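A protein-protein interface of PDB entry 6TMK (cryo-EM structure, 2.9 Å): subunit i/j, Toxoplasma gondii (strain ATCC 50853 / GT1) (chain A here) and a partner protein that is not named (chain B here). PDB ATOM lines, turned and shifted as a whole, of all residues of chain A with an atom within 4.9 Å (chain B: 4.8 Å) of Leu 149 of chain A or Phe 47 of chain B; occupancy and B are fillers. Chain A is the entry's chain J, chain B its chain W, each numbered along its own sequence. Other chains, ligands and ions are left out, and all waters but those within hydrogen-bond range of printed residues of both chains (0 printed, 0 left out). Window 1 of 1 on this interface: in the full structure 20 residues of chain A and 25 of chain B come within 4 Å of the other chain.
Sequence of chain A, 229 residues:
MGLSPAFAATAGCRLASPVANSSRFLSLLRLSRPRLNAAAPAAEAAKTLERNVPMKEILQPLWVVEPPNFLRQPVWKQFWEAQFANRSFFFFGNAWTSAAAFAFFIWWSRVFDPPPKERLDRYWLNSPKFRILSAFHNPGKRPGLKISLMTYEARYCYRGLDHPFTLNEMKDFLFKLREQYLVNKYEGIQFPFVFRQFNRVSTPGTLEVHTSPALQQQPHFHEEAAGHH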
ATOM      1  N   LEU A 145      11.257 -33.147  -2.454  1.00  0.00           N
ATOM      2  CA  LEU A 145       9.889 -32.651  -2.457  1.00  0.00           C
ATOM      3  C   LEU A 145       9.847 -31.133  -2.333  1.00  0.00           C
ATOM      4  O   LEU A 145       9.093 -30.460  -3.049  1.00  0.00           O
ATOM      5  CB  LEU A 145       9.125 -33.307  -1.314  1.00  0.00           C
ATOM      6  CG  LEU A 145       7.613 -33.172  -1.250  1.00  0.00           C
ATOM      7  CD1 LEU A 145       6.991 -33.717  -2.495  1.00  0.00           C
ATOM      8  CD2 LEU A 145       7.109 -33.901  -0.054  1.00  0.00           C
ATOM      9  N   LYS A 146      10.651 -30.577  -1.429  1.00  0.00           N
ATOM     10  CA  LYS A 146      10.734 -29.131  -1.309  1.00  0.00           C
ATOM     11  C   LYS A 146      11.298 -28.496  -2.572  1.00  0.00           C
ATOM     12  O   LYS A 146      10.929 -27.374  -2.919  1.00  0.00           O
ATOM     13  CB  LYS A 146      11.577 -28.761  -0.094  1.00  0.00           C
ATOM     14  CG  LYS A 146      11.068 -29.320   1.200  1.00  0.00           C
ATOM     15  CD  LYS A 146       9.652 -28.875   1.501  1.00  0.00           C
ATOM     16  CE  LYS A 146       9.276 -29.162   2.945  1.00  0.00           C
ATOM     17  NZ  LYS A 146       8.019 -28.495   3.362  1.00  0.00           N
ATOM     18  N   ILE A 147      12.182 -29.200  -3.273  1.00  0.00           N
ATOM     19  CA  ILE A 147      12.698 -28.702  -4.541  1.00  0.00           C
ATOM     20  C   ILE A 147      11.594 -28.671  -5.591  1.00  0.00           C
ATOM     21  O   ILE A 147      11.478 -27.713  -6.366  1.00  0.00           O
ATOM     22  CB  ILE A 147      13.899 -29.550  -4.986  1.00  0.00           C
ATOM     23  CG1 ILE A 147      15.089 -29.253  -4.080  1.00  0.00           C
ATOM     24  CG2 ILE A 147      14.260 -29.252  -6.419  1.00  0.00           C
ATOM     25  CD1 ILE A 147      16.151 -30.286  -4.092  1.00  0.00           C
ATOM     26  N   SER A 148      10.771 -29.718  -5.635  1.00  0.00           N
ATOM     27  CA  SER A 148       9.620 -29.719  -6.530  1.00  0.00           C
ATOM     28  C   SER A 148       8.703 -28.544  -6.226  1.00  0.00           C
ATOM     29  O   SER A 148       8.198 -27.882  -7.140  1.00  0.00           O
ATOM     30  CB  SER A 148       8.858 -31.033  -6.399  1.00  0.00           C
ATOM     31  OG  SER A 148       9.638 -32.122  -6.837  1.00  0.00           O
ATOM     32  N   LEU A 149       8.480 -28.272  -4.944  1.00  0.00           N
ATOM     33  CA  LEU A 149       7.599 -27.176  -4.570  1.00  0.00           C
ATOM     34  C   LEU A 149       8.226 -25.822  -4.883  1.00  0.00           C
ATOM     35  O   LEU A 149       7.512 -24.875  -5.221  1.00  0.00           O
ATOM     36  CB  LEU A 149       7.222 -27.290  -3.094  1.00  0.00           C
ATOM     37  CG  LEU A 149       6.403 -28.536  -2.769  1.00  0.00           C
ATOM     38  CD1 LEU A 149       6.313 -28.781  -1.294  1.00  0.00           C
ATOM     39  CD2 LEU A 149       5.025 -28.416  -3.341  1.00  0.00           C
ATOM     40  N   MET A 150       9.552 -25.719  -4.808  1.00  0.00           N
ATOM     41  CA  MET A 150      10.223 -24.489  -5.208  1.00  0.00           C
ATOM     42  C   MET A 150      10.096 -24.268  -6.706  1.00  0.00           C
ATOM     43  O   MET A 150       9.958 -23.130  -7.161  1.00  0.00           O
ATOM     44  CB  MET A 150      11.695 -24.538  -4.816  1.00  0.00           C
ATOM     45  CG  MET A 150      11.955 -24.377  -3.347  1.00  0.00           C
ATOM     46  SD  MET A 150      13.607 -24.885  -2.856  1.00  0.00           S
ATOM     47  CE  MET A 150      14.537 -23.463  -3.406  1.00  0.00           C
ATOM     48  N   THR A 151      10.176 -25.339  -7.491  1.00  0.00           N
ATOM     49  CA  THR A 151       9.933 -25.236  -8.926  1.00  0.00           C
ATOM     50  C   THR A 151       8.513 -24.760  -9.207  1.00  0.00           C
ATOM     51  O   THR A 151       8.290 -23.866 -10.036  1.00  0.00           O
ATOM     52  CB  THR A 151      10.197 -26.589  -9.585  1.00  0.00           C
ATOM     53  OG1 THR A 151      11.433 -27.132  -9.107  1.00  0.00           O
ATOM     54  CG2 THR A 151      10.247 -26.469 -11.073  1.00  0.00           C
ATOM     55  N   TYR A 152       7.537 -25.360  -8.526  1.00  0.00           N
ATOM     56  CA  TYR A 152       6.154 -24.925  -8.658  1.00  0.00           C
ATOM     57  C   TYR A 152       6.020 -23.441  -8.350  1.00  0.00           C
ATOM     58  O   TYR A 152       5.353 -22.702  -9.079  1.00  0.00           O
ATOM     59  CB  TYR A 152       5.259 -25.754  -7.740  1.00  0.00           C
ATOM     60  CG  TYR A 152       3.788 -25.619  -8.036  1.00  0.00           C
ATOM     61  CD1 TYR A 152       3.131 -26.537  -8.829  1.00  0.00           C
ATOM     62  CD2 TYR A 152       3.054 -24.580  -7.507  1.00  0.00           C
ATOM     63  CE1 TYR A 152       1.796 -26.416  -9.096  1.00  0.00           C
ATOM     64  CE2 TYR A 152       1.716 -24.451  -7.771  1.00  0.00           C
ATOM     65  CZ  TYR A 152       1.091 -25.369  -8.561  1.00  0.00           C
ATOM     66  OH  TYR A 152      -0.249 -25.231  -8.817  1.00  0.00           O
ATOM     67  N   GLU A 153       6.641 -22.994  -7.260  1.00  0.00           N
ATOM     68  CA  GLU A 153       6.627 -21.584  -6.897  1.00  0.00           C
ATOM     69  C   GLU A 153       7.233 -20.731  -7.999  1.00  0.00           C
ATOM     70  O   GLU A 153       6.631 -19.754  -8.447  1.00  0.00           O
ATOM     71  CB  GLU A 153       7.372 -21.389  -5.583  1.00  0.00           C
ATOM     72  CG  GLU A 153       7.451 -19.963  -5.101  1.00  0.00           C
ATOM     73  CD  GLU A 153       8.489 -19.787  -4.021  1.00  0.00           C
ATOM     74  OE1 GLU A 153       8.765 -20.771  -3.307  1.00  0.00           O
ATOM     75  OE2 GLU A 153       9.039 -18.673  -3.890  1.00  0.00           O
ATOM     76  N   PHE A 173       6.291 -35.489  -8.390  1.00  0.00           N
ATOM     77  CA  PHE A 173       5.869 -34.980  -7.090  1.00  0.00           C
ATOM     78  C   PHE A 173       5.267 -36.087  -6.234  1.00  0.00           C
ATOM     79  O   PHE A 173       5.600 -36.230  -5.050  1.00  0.00           O
ATOM     80  CB  PHE A 173       4.884 -33.829  -7.283  1.00  0.00           C
ATOM     81  CG  PHE A 173       4.145 -33.443  -6.043  1.00  0.00           C
ATOM     82  CD1 PHE A 173       4.746 -32.689  -5.062  1.00  0.00           C
ATOM     83  CD2 PHE A 173       2.831 -33.810  -5.875  1.00  0.00           C
ATOM     84  CE1 PHE A 173       4.059 -32.334  -3.934  1.00  0.00           C
ATOM     85  CE2 PHE A 173       2.143 -33.459  -4.749  1.00  0.00           C
ATOM     86  CZ  PHE A 173       2.752 -32.715  -3.782  1.00  0.00           C
ATOM     87  N   SER B  45      -3.775 -32.219  -8.685  1.00  0.00           N
ATOM     88  CA  SER B  45      -3.440 -30.919  -8.140  1.00  0.00           C
ATOM     89  C   SER B  45      -2.469 -31.098  -6.986  1.00  0.00           C
ATOM     90  O   SER B  45      -2.545 -32.071  -6.231  1.00  0.00           O
ATOM     91  CB  SER B  45      -4.687 -30.173  -7.665  1.00  0.00           C
ATOM     92  OG  SER B  45      -5.531 -29.848  -8.753  1.00  0.00           O
ATOM     93  N   VAL B  46      -1.554 -30.144  -6.858  1.00  0.00           N
ATOM     94  CA  VAL B  46      -0.549 -30.212  -5.806  1.00  0.00           C
ATOM     95  C   VAL B  46      -1.138 -29.780  -4.473  1.00  0.00           C
ATOM     96  O   VAL B  46      -1.106 -30.524  -3.487  1.00  0.00           O
ATOM     97  CB  VAL B  46       0.676 -29.360  -6.186  1.00  0.00           C
ATOM     98  CG1 VAL B  46       1.571 -29.147  -5.002  1.00  0.00           C
ATOM     99  CG2 VAL B  46       1.435 -30.026  -7.291  1.00  0.00           C
ATOM    100  N   PHE B  47      -1.683 -28.565  -4.421  1.00  0.00           N
ATOM    101  CA  PHE B  47      -2.143 -27.970  -3.176  1.00  0.00           C
ATOM    102  C   PHE B  47      -3.614 -28.245  -2.909  1.00  0.00           C
ATOM    103  O   PHE B  47      -4.284 -27.442  -2.249  1.00  0.00           O
ATOM    104  CB  PHE B  47      -1.871 -26.468  -3.191  1.00  0.00           C
ATOM    105  CG  PHE B  47      -0.418 -26.126  -3.152  1.00  0.00           C
ATOM    106  CD1 PHE B  47       0.216 -25.667  -4.283  1.00  0.00           C
ATOM    107  CD2 PHE B  47       0.318 -26.290  -1.997  1.00  0.00           C
ATOM    108  CE1 PHE B  47       1.551 -25.363  -4.262  1.00  0.00           C
ATOM    109  CE2 PHE B  47       1.654 -25.985  -1.970  1.00  0.00           C
ATOM    110  CZ  PHE B  47       2.274 -25.524  -3.106  1.00  0.00           C
ATOM    111  N   SER B  48      -4.137 -29.363  -3.408  1.00  0.00           N
ATOM    112  CA  SER B  48      -5.504 -29.753  -3.089  1.00  0.00           C
ATOM    113  C   SER B  48      -5.668 -30.016  -1.598  1.00  0.00           C
ATOM    114  O   SER B  48      -6.428 -29.328  -0.909  1.00  0.00           O
ATOM    115  CB  SER B  48      -5.890 -30.991  -3.894  1.00  0.00           C
ATOM    116  OG  SER B  48      -5.130 -32.108  -3.480  1.00  0.00           O
ATOM    117  N   GLN B  49      -4.955 -31.013  -1.084  1.00  0.00           N
ATOM    118  CA  GLN B  49      -5.078 -31.386   0.317  1.00  0.00           C
ATOM    119  C   GLN B  49      -4.032 -30.710   1.190  1.00  0.00           C
ATOM    120  O   GLN B  49      -4.356 -30.231   2.282  1.00  0.00           O
ATOM    121  CB  GLN B  49      -4.976 -32.906   0.465  1.00  0.00           C
ATOM    122  CG  GLN B  49      -5.196 -33.416   1.885  1.00  0.00           C
ATOM    123  CD  GLN B  49      -6.530 -32.989   2.464  1.00  0.00           C
ATOM    124  OE1 GLN B  49      -7.505 -33.741   2.427  1.00  0.00           O
ATOM    125  NE2 GLN B  49      -6.583 -31.776   3.005  1.00  0.00           N
ATOM    126  N   ILE B  50      -2.784 -30.656   0.739  1.00  0.00           N
ATOM    127  CA  ILE B  50      -1.735 -29.992   1.505  1.00  0.00           C
ATOM    128  C   ILE B  50      -1.990 -28.494   1.464  1.00  0.00           C
ATOM    129  O   ILE B  50      -2.624 -27.999   0.520  1.00  0.00           O
ATOM    130  CB  ILE B  50      -0.335 -30.317   0.965  1.00  0.00           C
ATOM    131  CG1 ILE B  50      -0.188 -29.850  -0.478  1.00  0.00           C
ATOM    132  CG2 ILE B  50      -0.088 -31.803   1.022  1.00  0.00           C
ATOM    133  CD1 ILE B  50       1.229 -29.848  -0.959  1.00  0.00           C
ATOM    134  N   PRO B  51      -1.511 -27.732   2.437  1.00  0.00           N
ATOM    135  CA  PRO B  51      -1.727 -26.289   2.417  1.00  0.00           C
ATOM    136  C   PRO B  51      -0.705 -25.569   1.548  1.00  0.00           C
ATOM    137  O   PRO B  51       0.348 -26.098   1.194  1.00  0.00           O
ATOM    138  CB  PRO B  51      -1.575 -25.907   3.889  1.00  0.00           C
ATOM    139  CG  PRO B  51      -0.556 -26.836   4.371  1.00  0.00           C
ATOM    140  CD  PRO B  51      -0.838 -28.146   3.678  1.00  0.00           C
ATOM    141  N   ASP B  52      -1.050 -24.327   1.216  1.00  0.00           N
ATOM    142  CA  ASP B  52      -0.204 -23.425   0.447  1.00  0.00           C
ATOM    143  C   ASP B  52       0.688 -22.569   1.330  1.00  0.00           C
ATOM    144  O   ASP B  52       1.084 -21.469   0.927  1.00  0.00           O
ATOM    145  CB  ASP B  52      -1.070 -22.536  -0.442  1.00  0.00           C
ATOM    146  CG  ASP B  52      -1.862 -21.520   0.352  1.00  0.00           C
ATOM    147  OD1 ASP B  52      -2.875 -21.910   0.972  1.00  0.00           O
ATOM    148  OD2 ASP B  52      -1.472 -20.334   0.359  1.00  0.00           O
ATOM    149  N   LEU B  55       4.365 -20.719   0.387  1.00  0.00           N
ATOM    150  CA  LEU B  55       4.407 -21.018  -1.036  1.00  0.00           C
ATOM    151  C   LEU B  55       5.373 -20.094  -1.762  1.00  0.00           C
ATOM    152  O   LEU B  55       6.254 -20.557  -2.495  1.00  0.00           O
ATOM    153  CB  LEU B  55       3.004 -20.908  -1.624  1.00  0.00           C
ATOM    154  CG  LEU B  55       2.851 -21.007  -3.143  1.00  0.00           C
ATOM    155  CD1 LEU B  55       3.667 -22.130  -3.725  1.00  0.00           C
ATOM    156  CD2 LEU B  55       1.397 -21.184  -3.497  1.00  0.00           C
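The side-chain carboxylate (OE1) of Glu 153 of chain A lies close to the backbone carbonyl oxygen (O) of Leu 55 of chain B, at 2.6 Å.
Among the printed residues, merely in contact across the chains: Leu 149 of chain A with Val 46 of chain B (3.9 Å), Leu 149 of chain A with Phe 47 of chain B (3.998 Å), Tyr 152 of chain A with Phe 47 of chain B (3.6 Å) and Phe 173 of chain A with Val 46 of chain B (3.95 Å).
Of the printed residues of chain B, Leu 149 of chain A touches Val 46 (3.9 Å) and Phe 47 (3.998 Å).
Of the printed residues of chain B, Tyr 152 of chain A touches Phe 47 (3.6 Å).
Of the printed residues of chain B, Phe 173 of chain A touches Val 46.
Of the printed residues of chain A, Val 46 of chain B touches Leu 149 (3.9 Å) and Phe 173 (3.95 Å).
Printed residues of chain A within 4 Å of Phe 47 of chain B: Leu 149 (3.998 Å) and Tyr 152 (3.6 Å).
Ser 48 of chain B touches none of the printed residues of chain A.
The nearest printed residue of chain B that does not touch Glu 153 of chain A is Phe 47 of chain B (6.4 Å).
Of the 10 printed residues of chain A, 4 touch a printed residue of chain B.
Hydrophobic or aromatic side chains of chain A that line the printed part of chain B: Leu 149, Tyr 152 and Phe 173.
Of the 9 printed residues of chain B, 3 touch a printed residue of chain A.
Printed residues of chain B that touch a printed residue of chain A: Val 46, Phe 47 and Leu 55.
Hydrophobic or aromatic side chains of chain B within 4 Å of the printed part of chain A: Val 46 and Phe 47.
Among the printed residues, 5 pairs touch across the chains.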
